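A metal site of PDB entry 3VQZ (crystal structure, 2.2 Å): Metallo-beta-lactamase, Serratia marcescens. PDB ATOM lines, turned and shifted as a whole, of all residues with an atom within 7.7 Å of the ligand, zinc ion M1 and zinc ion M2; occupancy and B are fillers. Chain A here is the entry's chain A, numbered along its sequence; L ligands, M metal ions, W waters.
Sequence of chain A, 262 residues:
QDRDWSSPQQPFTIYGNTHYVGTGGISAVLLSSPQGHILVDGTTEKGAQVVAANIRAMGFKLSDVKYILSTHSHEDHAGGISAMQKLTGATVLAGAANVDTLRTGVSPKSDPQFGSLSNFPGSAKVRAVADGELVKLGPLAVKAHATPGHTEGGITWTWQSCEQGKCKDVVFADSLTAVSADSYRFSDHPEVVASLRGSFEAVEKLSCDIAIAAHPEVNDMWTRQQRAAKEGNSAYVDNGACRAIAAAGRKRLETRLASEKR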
ATOM      1  N   TRP A   5     -14.915  -5.059 -18.955  1.00  0.00           N
ATOM      2  CA  TRP A   5     -14.520  -5.534 -17.614  1.00  0.00           C
ATOM      3  C   TRP A   5     -14.234  -4.438 -16.622  1.00  0.00           C
ATOM      4  O   TRP A   5     -14.343  -4.670 -15.407  1.00  0.00           O
ATOM      5  CB  TRP A   5     -13.304  -6.441 -17.702  1.00  0.00           C
ATOM      6  CG  TRP A   5     -13.529  -7.793 -18.354  1.00  0.00           C
ATOM      7  CD1 TRP A   5     -14.744  -8.398 -18.680  1.00  0.00           C
ATOM      8  CD2 TRP A   5     -12.500  -8.770 -18.735  1.00  0.00           C
ATOM      9  NE1 TRP A   5     -14.539  -9.642 -19.234  1.00  0.00           N
ATOM     10  CE2 TRP A   5     -13.216  -9.930 -19.296  1.00  0.00           C
ATOM     11  CE3 TRP A   5     -11.115  -8.804 -18.678  1.00  0.00           C
ATOM     12  CZ2 TRP A   5     -12.544 -11.044 -19.770  1.00  0.00           C
ATOM     13  CZ3 TRP A   5     -10.448  -9.943 -19.149  1.00  0.00           C
ATOM     14  CH2 TRP A   5     -11.154 -11.029 -19.683  1.00  0.00           C
ATOM     15  N   GLY A  25     -18.980  -5.216 -16.426  1.00  0.00           N
ATOM     16  CA  GLY A  25     -18.707  -6.571 -16.903  1.00  0.00           C
ATOM     17  C   GLY A  25     -18.277  -7.621 -15.879  1.00  0.00           C
ATOM     18  O   GLY A  25     -18.331  -8.808 -16.168  1.00  0.00           O
ATOM     19  N   ILE A  26     -17.844  -7.179 -14.692  1.00  0.00           N
ATOM     20  CA  ILE A  26     -17.401  -8.091 -13.614  1.00  0.00           C
ATOM     21  C   ILE A  26     -18.122  -7.778 -12.297  1.00  0.00           C
ATOM     22  O   ILE A  26     -18.179  -6.616 -11.860  1.00  0.00           O
ATOM     23  CB  ILE A  26     -15.862  -8.005 -13.383  1.00  0.00           C
ATOM     24  CG1 ILE A  26     -15.075  -8.257 -14.688  1.00  0.00           C
ATOM     25  CG2 ILE A  26     -15.405  -8.932 -12.270  1.00  0.00           C
ATOM     26  CD1 ILE A  26     -15.157  -9.684 -15.208  1.00  0.00           C
ATOM     27  N   THR A  71     -13.157 -15.170  -5.424  1.00  0.00           N
ATOM     28  CA  THR A  71     -13.720 -16.362  -6.072  1.00  0.00           C
ATOM     29  C   THR A  71     -12.568 -17.140  -6.693  1.00  0.00           C
ATOM     30  O   THR A  71     -12.211 -18.233  -6.213  1.00  0.00           O
ATOM     31  CB  THR A  71     -14.787 -16.002  -7.130  1.00  0.00           C
ATOM     32  OG1 THR A  71     -14.256 -15.076  -8.109  1.00  0.00           O
ATOM     33  CG2 THR A  71     -16.032 -15.415  -6.461  1.00  0.00           C
ATOM     34  N   HIS A  72     -11.962 -16.563  -7.724  1.00  0.00           N
ATOM     35  CA  HIS A  72     -10.776 -17.151  -8.346  1.00  0.00           C
ATOM     36  C   HIS A  72      -9.809 -16.100  -8.819  1.00  0.00           C
ATOM     37  O   HIS A  72     -10.179 -14.950  -9.085  1.00  0.00           O
ATOM     38  CB  HIS A  72     -11.141 -18.151  -9.451  1.00  0.00           C
ATOM     39  CG  HIS A  72     -11.616 -17.518 -10.740  1.00  0.00           C
ATOM     40  ND1 HIS A  72     -12.901 -17.210 -10.972  1.00  0.00           N
ATOM     41  CD2 HIS A  72     -10.922 -17.186 -11.910  1.00  0.00           C
ATOM     42  CE1 HIS A  72     -13.025 -16.695 -12.218  1.00  0.00           C
ATOM     43  NE2 HIS A  72     -11.825 -16.673 -12.782  1.00  0.00           N
ATOM     44  N   SER A  73      -8.548 -16.494  -8.915  1.00  0.00           N
ATOM     45  CA  SER A  73      -7.441 -15.564  -9.147  1.00  0.00           C
ATOM     46  C   SER A  73      -7.079 -15.370 -10.616  1.00  0.00           C
ATOM     47  O   SER A  73      -5.948 -15.679 -11.017  1.00  0.00           O
ATOM     48  CB  SER A  73      -6.207 -16.029  -8.373  1.00  0.00           C
ATOM     49  OG  SER A  73      -5.977 -17.410  -8.613  1.00  0.00           O
ATOM     50  N   HIS A  74      -8.029 -14.885 -11.412  1.00  0.00           N
ATOM     51  CA  HIS A  74      -7.751 -14.365 -12.755  1.00  0.00           C
ATOM     52  C   HIS A  74      -7.841 -12.874 -12.707  1.00  0.00           C
ATOM     53  O   HIS A  74      -8.529 -12.320 -11.832  1.00  0.00           O
ATOM     54  CB  HIS A  74      -8.729 -14.915 -13.786  1.00  0.00           C
ATOM     55  CG  HIS A  74      -8.484 -16.359 -14.152  1.00  0.00           C
ATOM     56  ND1 HIS A  74      -9.445 -17.160 -14.627  1.00  0.00           N
ATOM     57  CD2 HIS A  74      -7.324 -17.137 -14.083  1.00  0.00           C
ATOM     58  CE1 HIS A  74      -8.942 -18.387 -14.862  1.00  0.00           C
ATOM     59  NE2 HIS A  74      -7.636 -18.372 -14.523  1.00  0.00           N
ATOM     60  N   GLU A  75      -7.177 -12.217 -13.657  1.00  0.00           N
ATOM     61  CA  GLU A  75      -6.985 -10.761 -13.631  1.00  0.00           C
ATOM     62  C   GLU A  75      -8.279  -9.955 -13.623  1.00  0.00           C
ATOM     63  O   GLU A  75      -8.317  -8.859 -13.083  1.00  0.00           O
ATOM     64  CB  GLU A  75      -6.123 -10.312 -14.827  1.00  0.00           C
ATOM     65  CG  GLU A  75      -6.811 -10.514 -16.182  1.00  0.00           C
ATOM     66  CD  GLU A  75      -5.927 -10.169 -17.386  1.00  0.00           C
ATOM     67  OE1 GLU A  75      -5.096  -9.238 -17.290  1.00  0.00           O
ATOM     68  OE2 GLU A  75      -6.101 -10.813 -18.448  1.00  0.00           O
ATOM     69  N   ASP A  76      -9.327 -10.514 -14.214  1.00  0.00           N
ATOM     70  CA  ASP A  76     -10.577  -9.785 -14.339  1.00  0.00           C
ATOM     71  C   ASP A  76     -11.374  -9.719 -13.028  1.00  0.00           C
ATOM     72  O   ASP A  76     -12.178  -8.822 -12.885  1.00  0.00           O
ATOM     73  CB  ASP A  76     -11.436 -10.303 -15.518  1.00  0.00           C
ATOM     74  CG  ASP A  76     -11.704 -11.787 -15.469  1.00  0.00           C
ATOM     75  OD1 ASP A  76     -10.863 -12.528 -14.948  1.00  0.00           O
ATOM     76  OD2 ASP A  76     -12.765 -12.213 -15.952  1.00  0.00           O
ATOM     77  N   HIS A  77     -11.134 -10.637 -12.081  1.00  0.00           N
ATOM     78  CA  HIS A  77     -11.824 -10.660 -10.769  1.00  0.00           C
ATOM     79  C   HIS A  77     -10.943 -10.244  -9.642  1.00  0.00           C
ATOM     80  O   HIS A  77     -11.425  -9.715  -8.638  1.00  0.00           O
ATOM     81  CB  HIS A  77     -12.385 -12.040 -10.434  1.00  0.00           C
ATOM     82  CG  HIS A  77     -13.091 -12.666 -11.592  1.00  0.00           C
ATOM     83  ND1 HIS A  77     -14.393 -12.466 -11.841  1.00  0.00           N
ATOM     84  CD2 HIS A  77     -12.616 -13.450 -12.645  1.00  0.00           C
ATOM     85  CE1 HIS A  77     -14.746 -13.100 -12.979  1.00  0.00           C
ATOM     86  NE2 HIS A  77     -13.648 -13.707 -13.471  1.00  0.00           N
ATOM     87  N   ASP A 111      -2.938 -23.667 -14.000  1.00  0.00           N
ATOM     88  CA  ASP A 111      -4.058 -22.750 -14.302  1.00  0.00           C
ATOM     89  C   ASP A 111      -4.322 -22.673 -15.807  1.00  0.00           C
ATOM     90  O   ASP A 111      -3.423 -22.377 -16.576  1.00  0.00           O
ATOM     91  CB  ASP A 111      -3.740 -21.360 -13.718  1.00  0.00           C
ATOM     92  CG  ASP A 111      -4.788 -20.274 -14.046  1.00  0.00           C
ATOM     93  OD1 ASP A 111      -5.855 -20.535 -14.653  1.00  0.00           O
ATOM     94  OD2 ASP A 111      -4.543 -19.108 -13.690  1.00  0.00           O
ATOM     95  N   GLN A 113      -5.571 -20.433 -17.552  1.00  0.00           N
ATOM     96  CA  GLN A 113      -5.220 -19.117 -18.098  1.00  0.00           C
ATOM     97  C   GLN A 113      -3.844 -18.646 -17.649  1.00  0.00           C
ATOM     98  O   GLN A 113      -3.541 -17.461 -17.701  1.00  0.00           O
ATOM     99  CB  GLN A 113      -6.315 -18.072 -17.801  1.00  0.00           C
ATOM    100  CG  GLN A 113      -7.464 -18.152 -18.784  1.00  0.00           C
ATOM    101  CD  GLN A 113      -8.722 -17.459 -18.296  1.00  0.00           C
ATOM    102  OE1 GLN A 113      -8.658 -16.350 -17.743  1.00  0.00           O
ATOM    103  NE2 GLN A 113      -9.871 -18.106 -18.492  1.00  0.00           N
ATOM    104  N   HIS A 150     -12.054 -24.311 -12.926  1.00  0.00           N
ATOM    105  CA  HIS A 150     -11.737 -23.132 -13.714  1.00  0.00           C
ATOM    106  C   HIS A 150     -10.424 -22.575 -13.204  1.00  0.00           C
ATOM    107  O   HIS A 150      -9.600 -22.123 -13.992  1.00  0.00           O
ATOM    108  CB  HIS A 150     -12.865 -22.100 -13.641  1.00  0.00           C
ATOM    109  CG  HIS A 150     -12.587 -20.828 -14.408  1.00  0.00           C
ATOM    110  ND1 HIS A 150     -12.737 -20.743 -15.758  1.00  0.00           N
ATOM    111  CD2 HIS A 150     -12.130 -19.577 -13.984  1.00  0.00           C
ATOM    112  CE1 HIS A 150     -12.388 -19.501 -16.161  1.00  0.00           C
ATOM    113  NE2 HIS A 150     -12.041 -18.789 -15.080  1.00  0.00           N
ATOM    114  N   THR A 151     -10.231 -22.631 -11.894  1.00  0.00           N
ATOM    115  CA  THR A 151      -8.918 -22.525 -11.253  1.00  0.00           C
ATOM    116  C   THR A 151      -8.944 -23.571 -10.153  1.00  0.00           C
ATOM    117  O   THR A 151     -10.008 -24.049  -9.779  1.00  0.00           O
ATOM    118  CB  THR A 151      -8.649 -21.161 -10.580  1.00  0.00           C
ATOM    119  OG1 THR A 151      -9.546 -21.002  -9.467  1.00  0.00           O
ATOM    120  CG2 THR A 151      -8.821 -20.016 -11.548  1.00  0.00           C
ATOM    121  N   ASP A 174     -18.718 -18.689  -8.230  1.00  0.00           N
ATOM    122  CA  ASP A 174     -17.488 -18.700  -9.016  1.00  0.00           C
ATOM    123  C   ASP A 174     -17.758 -19.304 -10.405  1.00  0.00           C
ATOM    124  O   ASP A 174     -18.757 -20.040 -10.606  1.00  0.00           O
ATOM    125  CB  ASP A 174     -16.416 -19.481  -8.255  1.00  0.00           C
ATOM    126  CG  ASP A 174     -15.028 -19.307  -8.840  1.00  0.00           C
ATOM    127  OD1 ASP A 174     -14.748 -18.291  -9.521  1.00  0.00           O
ATOM    128  OD2 ASP A 174     -14.206 -20.210  -8.611  1.00  0.00           O
ATOM    129  N   SER A 175     -16.879 -18.994 -11.356  1.00  0.00           N
ATOM    130  CA  SER A 175     -16.969 -19.524 -12.726  1.00  0.00           C
ATOM    131  C   SER A 175     -16.740 -21.022 -12.808  1.00  0.00           C
ATOM    132  O   SER A 175     -15.812 -21.561 -12.176  1.00  0.00           O
ATOM    133  CB  SER A 175     -15.969 -18.833 -13.631  1.00  0.00           C
ATOM    134  OG  SER A 175     -16.131 -17.440 -13.539  1.00  0.00           O
ATOM    135  N   LEU A 176     -17.576 -21.679 -13.594  1.00  0.00           N
ATOM    136  CA  LEU A 176     -17.501 -23.120 -13.800  1.00  0.00           C
ATOM    137  C   LEU A 176     -17.203 -23.392 -15.281  1.00  0.00           C
ATOM    138  O   LEU A 176     -17.640 -24.404 -15.842  1.00  0.00           O
ATOM    139  CB  LEU A 176     -18.834 -23.772 -13.383  1.00  0.00           C
ATOM    140  CG  LEU A 176     -19.323 -23.506 -11.957  1.00  0.00           C
ATOM    141  CD1 LEU A 176     -20.675 -24.174 -11.725  1.00  0.00           C
ATOM    142  CD2 LEU A 176     -18.285 -23.990 -10.929  1.00  0.00           C
ATOM    143  N   THR A 177     -16.461 -22.479 -15.897  1.00  0.00           N
ATOM    144  CA  THR A 177     -16.262 -22.462 -17.343  1.00  0.00           C
ATOM    145  C   THR A 177     -14.962 -23.128 -17.790  1.00  0.00           C
ATOM    146  O   THR A 177     -13.868 -22.803 -17.305  1.00  0.00           O
ATOM    147  CB  THR A 177     -16.266 -21.012 -17.878  1.00  0.00           C
ATOM    148  OG1 THR A 177     -15.362 -20.228 -17.076  1.00  0.00           O
ATOM    149  CG2 THR A 177     -17.677 -20.416 -17.811  1.00  0.00           C
ATOM    150  N   ALA A 178     -15.104 -24.073 -18.715  1.00  0.00           N
ATOM    151  CA  ALA A 178     -13.950 -24.699 -19.353  1.00  0.00           C
ATOM    152  C   ALA A 178     -13.456 -23.772 -20.480  1.00  0.00           C
ATOM    153  O   ALA A 178     -13.692 -24.043 -21.659  1.00  0.00           O
ATOM    154  CB  ALA A 178     -14.321 -26.068 -19.909  1.00  0.00           C
ATOM    155  N   VAL A 179     -12.836 -22.666 -20.077  1.00  0.00           N
ATOM    156  CA  VAL A 179     -12.167 -21.737 -20.982  1.00  0.00           C
ATOM    157  C   VAL A 179     -10.731 -21.550 -20.482  1.00  0.00           C
ATOM    158  O   VAL A 179     -10.461 -21.729 -19.289  1.00  0.00           O
ATOM    159  CB  VAL A 179     -12.885 -20.354 -21.104  1.00  0.00           C
ATOM    160  CG1 VAL A 179     -14.288 -20.516 -21.653  1.00  0.00           C
ATOM    161  CG2 VAL A 179     -12.924 -19.587 -19.779  1.00  0.00           C
ATOM    162  N   SER A 180      -9.826 -21.197 -21.390  1.00  0.00           N
ATOM    163  CA  SER A 180      -8.406 -21.139 -21.077  1.00  0.00           C
ATOM    164  C   SER A 180      -7.646 -20.239 -22.054  1.00  0.00           C
ATOM    165  O   SER A 180      -8.254 -19.583 -22.899  1.00  0.00           O
ATOM    166  CB  SER A 180      -7.827 -22.543 -21.187  1.00  0.00           C
ATOM    167  OG  SER A 180      -7.926 -22.967 -22.532  1.00  0.00           O
ATOM    168  N   ALA A 214     -19.931 -14.527 -11.016  1.00  0.00           N
ATOM    169  CA  ALA A 214     -18.715 -13.721 -11.124  1.00  0.00           C
ATOM    170  C   ALA A 214     -18.728 -12.921 -12.442  1.00  0.00           C
ATOM    171  O   ALA A 214     -18.406 -11.729 -12.440  1.00  0.00           O
ATOM    172  CB  ALA A 214     -17.470 -14.584 -10.986  1.00  0.00           C
ATOM    173  N   HIS A 215     -19.116 -13.578 -13.541  1.00  0.00           N
ATOM    174  CA  HIS A 215     -19.523 -12.860 -14.763  1.00  0.00           C
ATOM    175  C   HIS A 215     -21.022 -12.637 -14.728  1.00  0.00           C
ATOM    176  O   HIS A 215     -21.780 -13.547 -15.017  1.00  0.00           O
ATOM    177  CB  HIS A 215     -19.067 -13.574 -16.043  1.00  0.00           C
ATOM    178  CG  HIS A 215     -17.577 -13.444 -16.305  1.00  0.00           C
ATOM    179  ND1 HIS A 215     -17.059 -12.498 -17.144  1.00  0.00           N
ATOM    180  CD2 HIS A 215     -16.488 -14.159 -15.801  1.00  0.00           C
ATOM    181  CE1 HIS A 215     -15.706 -12.609 -17.155  1.00  0.00           C
ATOM    182  NE2 HIS A 215     -15.355 -13.616 -16.324  1.00  0.00           N
ATOM    183  N   GLU A 217     -23.604 -11.525 -16.294  1.00  0.00           N
ATOM    184  CA  GLU A 217     -24.573 -11.957 -17.335  1.00  0.00           C
ATOM    185  C   GLU A 217     -24.847 -13.474 -17.333  1.00  0.00           C
ATOM    186  O   GLU A 217     -25.818 -13.939 -17.937  1.00  0.00           O
ATOM    187  CB  GLU A 217     -24.141 -11.458 -18.736  1.00  0.00           C
ATOM    188  CG  GLU A 217     -22.951 -12.189 -19.364  1.00  0.00           C
ATOM    189  CD  GLU A 217     -21.591 -11.850 -18.757  1.00  0.00           C
ATOM    190  OE1 GLU A 217     -21.454 -10.877 -17.991  1.00  0.00           O
ATOM    191  OE2 GLU A 217     -20.613 -12.558 -19.061  1.00  0.00           O
ATOM    192  N   VAL A 218     -24.003 -14.241 -16.639  1.00  0.00           N
ATOM    193  CA  VAL A 218     -24.201 -15.669 -16.547  1.00  0.00           C
ATOM    194  C   VAL A 218     -25.522 -15.999 -15.813  1.00  0.00           C
ATOM    195  O   VAL A 218     -26.111 -17.063 -16.025  1.00  0.00           O
ATOM    196  CB  VAL A 218     -22.980 -16.393 -15.924  1.00  0.00           C
ATOM    197  CG1 VAL A 218     -23.270 -17.865 -15.676  1.00  0.00           C
ATOM    198  CG2 VAL A 218     -21.760 -16.234 -16.842  1.00  0.00           C
ATOM    199  N   ARG A 252     -21.011 -26.637 -21.706  1.00  0.00           N
ATOM    200  CA  ARG A 252     -19.806 -25.982 -22.209  1.00  0.00           C
ATOM    201  C   ARG A 252     -18.551 -26.877 -22.181  1.00  0.00           C
ATOM    202  O   ARG A 252     -17.774 -26.887 -23.125  1.00  0.00           O
ATOM    203  CB  ARG A 252     -19.564 -24.650 -21.493  1.00  0.00           C
ATOM    204  CG  ARG A 252     -18.326 -23.916 -21.987  1.00  0.00           C
ATOM    205  CD  ARG A 252     -17.916 -22.799 -21.046  1.00  0.00           C
ATOM    206  NE  ARG A 252     -18.669 -21.559 -21.262  1.00  0.00           N
ATOM    207  CZ  ARG A 252     -18.615 -20.819 -22.366  1.00  0.00           C
ATOM    208  NH1 ARG A 252     -17.865 -21.203 -23.401  1.00  0.00           N
ATOM    209  NH2 ARG A 252     -19.309 -19.699 -22.448  1.00  0.00           N
HETATM  210  O1  LIG L   1     -15.421 -17.548 -16.891  1.00  0.00           O
HETATM  211  C1  LIG L   1     -14.506 -16.812 -16.438  1.00  0.00           C
HETATM  212  O2  LIG L   1     -14.463 -16.466 -15.232  1.00  0.00           O
HETATM  213  C2  LIG L   1     -13.434 -16.327 -17.390  1.00  0.00           C
HETATM  214  S1  LIG L   1     -12.064 -15.552 -16.486  1.00  0.00           S
HETATM  215 ZN    ZN M   1     -11.426 -16.834 -14.844  1.00  0.00          ZN
HETATM  216 ZN    ZN M   2     -13.590 -14.029 -15.458  1.00  0.00          ZN
HETATM  217  O   HOH W   1     -18.339 -17.585 -16.169  1.00  0.00           O
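OG1 of Thr 177 is in hydrogen-bond range of O1 of the ligand.
An oxygen (O1) of the ligand lies close to the side-chain hydroxyl (OG) of Ser 175.
A sulfur (S1) of the ligand lies close to the side-chain amide oxygen of Gln 113 (3.7 Å).
The side-chain carboxylate of Asp 174 sits at hydrogen-bond distance from a ring nitrogen (ND1) of His 72.
NE2 of His 74 sits at hydrogen-bond distance from OD1 of Asp 111.
OE1 of Gln 113 sits close to ND1 of His 74 (3.3 Å).
The backbone NH (N) of Gln 113 lies within hydrogen-bond range of the side-chain carboxylate (OD1) of Asp 111, 2.9 Å away.
A ring nitrogen (ND1) of His 150 sits at hydrogen-bond distance from the backbone carbonyl oxygen of Thr 177 (2.8 Å).
Hydrophobic or aromatic side chains within 4 Å of the ligand: His 72, His 150 and His 215.
Along chain A the residues within 4 Å of the ligand span positions 72 to 215.
Within 4 Å of zinc ion M1: His 72, His 74 and His 150.
Along chain A the residues within 4 Å of zinc ion M1 span positions 72 to 150.
Within 4 Å of zinc ion M2: Asp 76, His 77 and His 215.
Zinc ion M1 is bound by ND1 of His 74 (2.0 Å), NE2 of His 150 (2.1 Å), NE2 of His 72 (2.1 Å) and S1 of the ligand (2.2 Å).
Zinc ion M1 has four donor atoms within binding distance.
A ring nitrogen (NE2) of His 215 is bound to zinc ion M2 (2.0 Å).
A ring nitrogen (NE2) of His 77 binds zinc ion M2.
The side-chain carboxylate (OD2) of Asp 76 is bound to zinc ion M2, 2.1 Å away.
Zinc ion M2 is bound by S1 of the ligand, 2.4 Å away.
O2 of the ligand is bound to zinc ion M2 (2.6 Å).
Water W1 lies within hydrogen-bond range of O1 of the ligand (3.0 Å) and OG of Ser 175 (3.4 Å).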
